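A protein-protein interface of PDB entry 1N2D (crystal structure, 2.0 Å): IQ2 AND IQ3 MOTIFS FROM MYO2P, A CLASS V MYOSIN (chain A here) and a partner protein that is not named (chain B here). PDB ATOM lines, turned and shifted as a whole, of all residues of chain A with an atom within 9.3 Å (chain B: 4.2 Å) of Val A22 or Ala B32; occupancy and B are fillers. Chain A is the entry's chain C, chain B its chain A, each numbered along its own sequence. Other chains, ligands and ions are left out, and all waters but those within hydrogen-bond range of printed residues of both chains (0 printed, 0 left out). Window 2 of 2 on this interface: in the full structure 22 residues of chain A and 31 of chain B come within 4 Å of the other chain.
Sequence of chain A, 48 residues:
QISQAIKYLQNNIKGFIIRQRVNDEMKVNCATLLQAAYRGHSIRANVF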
ATOM      1  N   LYS A  14      18.220   3.349   1.251  1.00  0.00           N
ATOM      2  CA  LYS A  14      18.643   2.611   2.437  1.00  0.00           C
ATOM      3  C   LYS A  14      20.028   3.089   2.886  1.00  0.00           C
ATOM      4  O   LYS A  14      20.283   3.232   4.078  1.00  0.00           O
ATOM      5  CB  LYS A  14      18.673   1.110   2.148  1.00  0.00           C
ATOM      6  CG  LYS A  14      17.284   0.490   2.075  1.00  0.00           C
ATOM      7  CD  LYS A  14      17.329  -0.891   1.438  1.00  0.00           C
ATOM      8  CE  LYS A  14      17.127  -1.990   2.455  1.00  0.00           C
ATOM      9  NZ  LYS A  14      15.766  -1.935   3.059  1.00  0.00           N
ATOM     10  N   GLY A  15      20.922   3.335   1.930  1.00  0.00           N
ATOM     11  CA  GLY A  15      22.248   3.819   2.278  1.00  0.00           C
ATOM     12  C   GLY A  15      22.127   5.195   2.917  1.00  0.00           C
ATOM     13  O   GLY A  15      22.777   5.489   3.919  1.00  0.00           O
ATOM     14  N   PHE A  16      21.283   6.039   2.332  1.00  0.00           N
ATOM     15  CA  PHE A  16      21.057   7.387   2.848  1.00  0.00           C
ATOM     16  C   PHE A  16      20.527   7.374   4.286  1.00  0.00           C
ATOM     17  O   PHE A  16      20.986   8.139   5.139  1.00  0.00           O
ATOM     18  CB  PHE A  16      20.062   8.125   1.949  1.00  0.00           C
ATOM     19  CG  PHE A  16      19.713   9.512   2.431  1.00  0.00           C
ATOM     20  CD1 PHE A  16      20.539  10.592   2.143  1.00  0.00           C
ATOM     21  CD2 PHE A  16      18.567   9.728   3.192  1.00  0.00           C
ATOM     22  CE1 PHE A  16      20.231  11.878   2.606  1.00  0.00           C
ATOM     23  CE2 PHE A  16      18.248  11.007   3.660  1.00  0.00           C
ATOM     24  CZ  PHE A  16      19.084  12.084   3.364  1.00  0.00           C
ATOM     25  N   ILE A  17      19.562   6.500   4.550  1.00  0.00           N
ATOM     26  CA  ILE A  17      18.954   6.396   5.874  1.00  0.00           C
ATOM     27  C   ILE A  17      19.952   5.985   6.942  1.00  0.00           C
ATOM     28  O   ILE A  17      19.997   6.582   8.017  1.00  0.00           O
ATOM     29  CB  ILE A  17      17.791   5.380   5.868  1.00  0.00           C
ATOM     30  CG1 ILE A  17      16.632   5.932   5.038  1.00  0.00           C
ATOM     31  CG2 ILE A  17      17.370   5.061   7.292  1.00  0.00           C
ATOM     32  CD1 ILE A  17      15.489   4.948   4.850  1.00  0.00           C
ATOM     33  N   ILE A  18      20.754   4.966   6.652  1.00  0.00           N
ATOM     34  CA  ILE A  18      21.732   4.508   7.621  1.00  0.00           C
ATOM     35  C   ILE A  18      22.747   5.591   7.930  1.00  0.00           C
ATOM     36  O   ILE A  18      23.055   5.846   9.095  1.00  0.00           O
ATOM     37  CB  ILE A  18      22.476   3.248   7.132  1.00  0.00           C
ATOM     38  CG1 ILE A  18      21.485   2.094   6.956  1.00  0.00           C
ATOM     39  CG2 ILE A  18      23.562   2.866   8.135  1.00  0.00           C
ATOM     40  CD1 ILE A  18      20.694   1.731   8.226  1.00  0.00           C
ATOM     41  N   ARG A  19      23.260   6.232   6.887  1.00  0.00           N
ATOM     42  CA  ARG A  19      24.245   7.283   7.075  1.00  0.00           C
ATOM     43  C   ARG A  19      23.670   8.456   7.874  1.00  0.00           C
ATOM     44  O   ARG A  19      24.367   9.064   8.698  1.00  0.00           O
ATOM     45  CB  ARG A  19      24.782   7.735   5.713  1.00  0.00           C
ATOM     46  CG  ARG A  19      25.578   6.617   5.002  1.00  0.00           C
ATOM     47  CD  ARG A  19      26.284   7.109   3.741  1.00  0.00           C
ATOM     48  NE  ARG A  19      25.393   7.279   2.589  1.00  0.00           N
ATOM     49  CZ  ARG A  19      25.067   6.308   1.736  1.00  0.00           C
ATOM     50  NH1 ARG A  19      25.552   5.079   1.893  1.00  0.00           N
ATOM     51  NH2 ARG A  19      24.272   6.570   0.704  1.00  0.00           N
ATOM     52  N   GLN A  20      22.398   8.764   7.644  1.00  0.00           N
ATOM     53  CA  GLN A  20      21.743   9.843   8.374  1.00  0.00           C
ATOM     54  C   GLN A  20      21.615   9.415   9.833  1.00  0.00           C
ATOM     55  O   GLN A  20      21.894  10.185  10.758  1.00  0.00           O
ATOM     56  CB  GLN A  20      20.355  10.113   7.776  1.00  0.00           C
ATOM     57  CG  GLN A  20      19.487  11.075   8.573  1.00  0.00           C
ATOM     58  CD  GLN A  20      18.177  11.381   7.862  1.00  0.00           C
ATOM     59  OE1 GLN A  20      18.122  12.226   6.962  1.00  0.00           O
ATOM     60  NE2 GLN A  20      17.121  10.678   8.247  1.00  0.00           N
ATOM     61  N   ARG A  21      21.201   8.169  10.032  1.00  0.00           N
ATOM     62  CA  ARG A  21      21.025   7.631  11.372  1.00  0.00           C
ATOM     63  C   ARG A  21      22.341   7.666  12.146  1.00  0.00           C
ATOM     64  O   ARG A  21      22.384   8.101  13.296  1.00  0.00           O
ATOM     65  CB  ARG A  21      20.506   6.199  11.288  1.00  0.00           C
ATOM     66  CG  ARG A  21      20.131   5.593  12.624  1.00  0.00           C
ATOM     67  CD  ARG A  21      19.719   4.137  12.448  1.00  0.00           C
ATOM     68  NE  ARG A  21      18.533   3.990  11.607  1.00  0.00           N
ATOM     69  CZ  ARG A  21      18.131   2.834  11.086  1.00  0.00           C
ATOM     70  NH1 ARG A  21      18.821   1.723  11.314  1.00  0.00           N
ATOM     71  NH2 ARG A  21      17.041   2.784  10.336  1.00  0.00           N
ATOM     72  N   VAL A  22      23.411   7.209  11.506  1.00  0.00           N
ATOM     73  CA  VAL A  22      24.729   7.195  12.123  1.00  0.00           C
ATOM     74  C   VAL A  22      25.196   8.609  12.461  1.00  0.00           C
ATOM     75  O   VAL A  22      25.719   8.853  13.542  1.00  0.00           O
ATOM     76  CB  VAL A  22      25.758   6.522  11.188  1.00  0.00           C
ATOM     77  CG1 VAL A  22      27.171   6.784  11.676  1.00  0.00           C
ATOM     78  CG2 VAL A  22      25.503   5.026  11.143  1.00  0.00           C
ATOM     79  N   ASN A  23      25.000   9.534  11.526  1.00  0.00           N
ATOM     80  CA  ASN A  23      25.391  10.923  11.717  1.00  0.00           C
ATOM     81  C   ASN A  23      24.646  11.507  12.921  1.00  0.00           C
ATOM     82  O   ASN A  23      25.234  12.209  13.756  1.00  0.00           O
ATOM     83  CB  ASN A  23      25.075  11.716  10.435  1.00  0.00           C
ATOM     84  CG  ASN A  23      25.639  13.127  10.459  1.00  0.00           C
ATOM     85  OD1 ASN A  23      24.893  14.104  10.511  1.00  0.00           O
ATOM     86  ND2 ASN A  23      26.964  13.239  10.418  1.00  0.00           N
ATOM     87  N   ASP A  24      23.351  11.216  13.022  1.00  0.00           N
ATOM     88  CA  ASP A  24      22.576  11.719  14.145  1.00  0.00           C
ATOM     89  C   ASP A  24      23.061  11.118  15.466  1.00  0.00           C
ATOM     90  O   ASP A  24      23.136  11.820  16.478  1.00  0.00           O
ATOM     91  CB  ASP A  24      21.083  11.441  13.945  1.00  0.00           C
ATOM     92  CG  ASP A  24      20.454  12.389  12.934  1.00  0.00           C
ATOM     93  OD1 ASP A  24      21.005  13.501  12.746  1.00  0.00           O
ATOM     94  OD2 ASP A  24      19.413  12.036  12.340  1.00  0.00           O
ATOM     95  N   GLU A  25      23.394   9.828  15.462  1.00  0.00           N
ATOM     96  CA  GLU A  25      23.897   9.193  16.679  1.00  0.00           C
ATOM     97  C   GLU A  25      25.219   9.829  17.095  1.00  0.00           C
ATOM     98  O   GLU A  25      25.480  10.031  18.281  1.00  0.00           O
ATOM     99  CB  GLU A  25      24.112   7.694  16.468  1.00  0.00           C
ATOM    100  CG  GLU A  25      22.836   6.884  16.431  1.00  0.00           C
ATOM    101  CD  GLU A  25      23.100   5.402  16.191  1.00  0.00           C
ATOM    102  OE1 GLU A  25      24.016   4.850  16.846  1.00  0.00           O
ATOM    103  OE2 GLU A  25      22.387   4.795  15.359  1.00  0.00           O
ATOM    104  N   MET A  26      26.067  10.131  16.116  1.00  0.00           N
ATOM    105  CA  MET A  26      27.347  10.751  16.418  1.00  0.00           C
ATOM    106  C   MET A  26      27.121  12.142  16.997  1.00  0.00           C
ATOM    107  O   MET A  26      27.861  12.582  17.875  1.00  0.00           O
ATOM    108  CB  MET A  26      28.207  10.838  15.157  1.00  0.00           C
ATOM    109  CG  MET A  26      28.892   9.523  14.808  1.00  0.00           C
ATOM    110  SD  MET A  26      29.586   9.538  13.146  1.00  0.00           S
ATOM    111  CE  MET A  26      30.867  10.788  13.314  1.00  0.00           C
ATOM    112  N   LYS A  27      26.103  12.840  16.501  1.00  0.00           N
ATOM    113  CA  LYS A  27      25.811  14.167  17.022  1.00  0.00           C
ATOM    114  C   LYS A  27      25.348  14.044  18.465  1.00  0.00           C
ATOM    115  O   LYS A  27      25.809  14.789  19.331  1.00  0.00           O
ATOM    116  CB  LYS A  27      24.743  14.861  16.177  1.00  0.00           C
ATOM    117  CG  LYS A  27      25.256  15.359  14.832  1.00  0.00           C
ATOM    118  CD  LYS A  27      24.134  15.996  14.016  1.00  0.00           C
ATOM    119  CE  LYS A  27      24.648  16.548  12.687  1.00  0.00           C
ATOM    120  NZ  LYS A  27      23.546  17.120  11.854  1.00  0.00           N
ATOM    121  N   VAL A  28      24.448  13.096  18.729  1.00  0.00           N
ATOM    122  CA  VAL A  28      23.948  12.886  20.088  1.00  0.00           C
ATOM    123  C   VAL A  28      25.079  12.498  21.035  1.00  0.00           C
ATOM    124  O   VAL A  28      25.167  13.027  22.148  1.00  0.00           O
ATOM    125  CB  VAL A  28      22.868  11.784  20.144  1.00  0.00           C
ATOM    126  CG1 VAL A  28      22.585  11.411  21.601  1.00  0.00           C
ATOM    127  CG2 VAL A  28      21.582  12.272  19.486  1.00  0.00           C
ATOM    128  N   ASN A  29      25.938  11.578  20.597  1.00  0.00           N
ATOM    129  CA  ASN A  29      27.066  11.144  21.418  1.00  0.00           C
ATOM    130  C   ASN A  29      27.990  12.312  21.729  1.00  0.00           C
ATOM    131  O   ASN A  29      28.465  12.451  22.854  1.00  0.00           O
ATOM    132  CB  ASN A  29      27.890  10.057  20.718  1.00  0.00           C
ATOM    133  CG  ASN A  29      27.120   8.768  20.515  1.00  0.00           C
ATOM    134  OD1 ASN A  29      26.161   8.475  21.230  1.00  0.00           O
ATOM    135  ND2 ASN A  29      27.553   7.978  19.543  1.00  0.00           N
ATOM    136  N   CYS A  30      28.256  13.144  20.725  1.00  0.00           N
ATOM    137  CA  CYS A  30      29.129  14.301  20.911  1.00  0.00           C
ATOM    138  C   CYS A  30      28.543  15.256  21.952  1.00  0.00           C
ATOM    139  O   CYS A  30      29.243  15.714  22.854  1.00  0.00           O
ATOM    140  CB  CYS A  30      29.313  15.048  19.586  1.00  0.00           C
ATOM    141  SG  CYS A  30      30.255  16.596  19.722  1.00  0.00           S
ATOM    142  N   ILE B   9      33.156   4.147  13.009  1.00  0.00           N
ATOM    143  CA  ILE B   9      31.799   3.746  12.673  1.00  0.00           C
ATOM    144  C   ILE B   9      31.639   2.322  13.191  1.00  0.00           C
ATOM    145  O   ILE B   9      30.612   1.970  13.777  1.00  0.00           O
ATOM    146  CB  ILE B   9      31.539   3.824  11.144  1.00  0.00           C
ATOM    147  CG1 ILE B   9      31.462   5.300  10.719  1.00  0.00           C
ATOM    148  CG2 ILE B   9      30.235   3.128  10.793  1.00  0.00           C
ATOM    149  CD1 ILE B   9      31.294   5.532   9.217  1.00  0.00           C
ATOM    150  N   PHE B  13      28.970   0.655  15.914  1.00  0.00           N
ATOM    151  CA  PHE B  13      28.108  -0.511  15.726  1.00  0.00           C
ATOM    152  C   PHE B  13      28.347  -1.572  16.795  1.00  0.00           C
ATOM    153  O   PHE B  13      27.432  -2.299  17.184  1.00  0.00           O
ATOM    154  CB  PHE B  13      28.345  -1.146  14.356  1.00  0.00           C
ATOM    155  CG  PHE B  13      27.529  -0.541  13.256  1.00  0.00           C
ATOM    156  CD1 PHE B  13      27.800   0.740  12.792  1.00  0.00           C
ATOM    157  CD2 PHE B  13      26.491  -1.264  12.670  1.00  0.00           C
ATOM    158  CE1 PHE B  13      27.051   1.296  11.758  1.00  0.00           C
ATOM    159  CE2 PHE B  13      25.732  -0.715  11.631  1.00  0.00           C
ATOM    160  CZ  PHE B  13      26.013   0.562  11.177  1.00  0.00           C
ATOM    161  N   ASP B  28      24.213  -2.846   6.937  1.00  0.00           N
ATOM    162  CA  ASP B  28      24.089  -1.492   7.457  1.00  0.00           C
ATOM    163  C   ASP B  28      25.442  -0.849   7.681  1.00  0.00           C
ATOM    164  O   ASP B  28      25.595   0.358   7.492  1.00  0.00           O
ATOM    165  CB  ASP B  28      23.247  -1.495   8.732  1.00  0.00           C
ATOM    166  CG  ASP B  28      21.763  -1.686   8.434  1.00  0.00           C
ATOM    167  OD1 ASP B  28      20.966  -1.846   9.374  1.00  0.00           O
ATOM    168  OD2 ASP B  28      21.397  -1.666   7.240  1.00  0.00           O
ATOM    169  N   TYR B  29      26.430  -1.652   8.064  1.00  0.00           N
ATOM    170  CA  TYR B  29      27.772  -1.121   8.250  1.00  0.00           C
ATOM    171  C   TYR B  29      28.318  -0.698   6.878  1.00  0.00           C
ATOM    172  O   TYR B  29      28.955   0.349   6.743  1.00  0.00           O
ATOM    173  CB  TYR B  29      28.701  -2.172   8.863  1.00  0.00           C
ATOM    174  CG  TYR B  29      30.118  -1.670   8.980  1.00  0.00           C
ATOM    175  CD1 TYR B  29      30.473  -0.737   9.958  1.00  0.00           C
ATOM    176  CD2 TYR B  29      31.097  -2.090   8.082  1.00  0.00           C
ATOM    177  CE1 TYR B  29      31.775  -0.239  10.036  1.00  0.00           C
ATOM    178  CE2 TYR B  29      32.396  -1.599   8.145  1.00  0.00           C
ATOM    179  CZ  TYR B  29      32.729  -0.679   9.123  1.00  0.00           C
ATOM    180  OH  TYR B  29      34.015  -0.206   9.179  1.00  0.00           O
ATOM    181  N   LEU B  30      28.062  -1.513   5.856  1.00  0.00           N
ATOM    182  CA  LEU B  30      28.535  -1.190   4.509  1.00  0.00           C
ATOM    183  C   LEU B  30      27.867   0.097   4.030  1.00  0.00           C
ATOM    184  O   LEU B  30      28.485   0.925   3.353  1.00  0.00           O
ATOM    185  CB  LEU B  30      28.237  -2.347   3.557  1.00  0.00           C
ATOM    186  CG  LEU B  30      29.045  -3.618   3.858  1.00  0.00           C
ATOM    187  CD1 LEU B  30      28.626  -4.724   2.924  1.00  0.00           C
ATOM    188  CD2 LEU B  30      30.537  -3.334   3.703  1.00  0.00           C
ATOM    189  N   ARG B  31      26.600   0.267   4.390  1.00  0.00           N
ATOM    190  CA  ARG B  31      25.873   1.475   4.027  1.00  0.00           C
ATOM    191  C   ARG B  31      26.447   2.661   4.804  1.00  0.00           C
ATOM    192  O   ARG B  31      26.676   3.739   4.249  1.00  0.00           O
ATOM    193  CB  ARG B  31      24.386   1.292   4.346  1.00  0.00           C
ATOM    194  CG  ARG B  31      23.726   0.300   3.409  1.00  0.00           C
ATOM    195  CD  ARG B  31      22.309  -0.078   3.826  1.00  0.00           C
ATOM    196  NE  ARG B  31      21.765  -1.057   2.887  1.00  0.00           N
ATOM    197  CZ  ARG B  31      21.357  -2.277   3.220  1.00  0.00           C
ATOM    198  NH1 ARG B  31      21.414  -2.680   4.486  1.00  0.00           N
ATOM    199  NH2 ARG B  31      20.931  -3.112   2.280  1.00  0.00           N
ATOM    200  N   ALA B  32      26.700   2.442   6.090  1.00  0.00           N
ATOM    201  CA  ALA B  32      27.229   3.479   6.955  1.00  0.00           C
ATOM    202  C   ALA B  32      28.554   4.034   6.439  1.00  0.00           C
ATOM    203  O   ALA B  32      28.779   5.244   6.473  1.00  0.00           O
ATOM    204  CB  ALA B  32      27.402   2.933   8.369  1.00  0.00           C
ATOM    205  N   ILE B  33      29.424   3.155   5.943  1.00  0.00           N
ATOM    206  CA  ILE B  33      30.720   3.601   5.449  1.00  0.00           C
ATOM    207  C   ILE B  33      30.693   4.163   4.024  1.00  0.00           C
ATOM    208  O   ILE B  33      31.734   4.566   3.498  1.00  0.00           O
ATOM    209  CB  ILE B  33      31.783   2.473   5.551  1.00  0.00           C
ATOM    210  CG1 ILE B  33      31.378   1.283   4.683  1.00  0.00           C
ATOM    211  CG2 ILE B  33      31.932   2.024   7.013  1.00  0.00           C
ATOM    212  CD1 ILE B  33      32.409   0.173   4.667  1.00  0.00           C
ATOM    213  N   GLY B  34      29.522   4.181   3.390  1.00  0.00           N
ATOM    214  CA  GLY B  34      29.447   4.769   2.063  1.00  0.00           C
ATOM    215  C   GLY B  34      28.925   3.977   0.881  1.00  0.00           C
ATOM    216  O   GLY B  34      28.760   4.552  -0.192  1.00  0.00           O
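Val A22 touches one residue of chain B.
Of chain A, only Ile A18, Arg A19 and Val A22 come within 4 Å of Ala B32.
Printed residues of chain A within 4 Å of Arg B31: Lys A14 (3.8 Å), Gly A15 (3.9 Å), Ile A18 (3.9 Å) and Arg A19 (2.9 Å).
Of the printed residues of chain B, Arg A19 touches Arg B31 (2.9 Å), Ala B32 (3.8 Å) and Gly B34 (3.7 Å).
Printed residues of chain B within 4 Å of Lys A14: Arg B31.
Of the printed residues of chain B, Ile A18 touches Asp B28 (3.3 Å), Arg B31 (3.9 Å) and Ala B32 (3.8 Å).
Gln A20 touches none of the printed residues of chain B.
Ile A17 touches none of the printed residues of chain B.
The nearest residue of chain B that does not touch Val A22 is Phe B13 (4.1 Å).
The nearest residue of chain A that does not touch Ala B32 is Gly A15 (5.4 Å).
The nearest printed residue of chain A that does not touch Gly B34 is Gly A15 (6.8 Å).
NE of Arg B31 touches CB of Lys A14 (3.8 Å).
Gly A15 touches Arg B31 (CA to CB, 3.9 Å).
Ile A18 touches Asp B28 (CG2 to O, 3.3 Å).
Ile A18 touches Arg B31.
Ile A18 touches Ala B32 (CG2 to N, 3.8 Å).
Ala B32 touches Arg A19.
Gly B34 touches Arg A19.
Val A22 touches Ala B32.
The backbone carbonyl oxygen (O) of Arg B31 is in hydrogen-bond range of the guanidinium group (NH1) of Arg A19.
Of the 17 printed residues of chain A, 5 touch a printed residue of chain B.
Of the 9 printed residues of chain B, 4 touch a printed residue of chain A.
The side-chain carboxylate of Asp B28 lies within salt-bridge range of the guanidinium group of Arg B31, at 2.9 Å.
The backbone carbonyl oxygen (O) of Gly A15 sits close to the guanidinium group (NE) of Arg A19 (3.4 Å).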
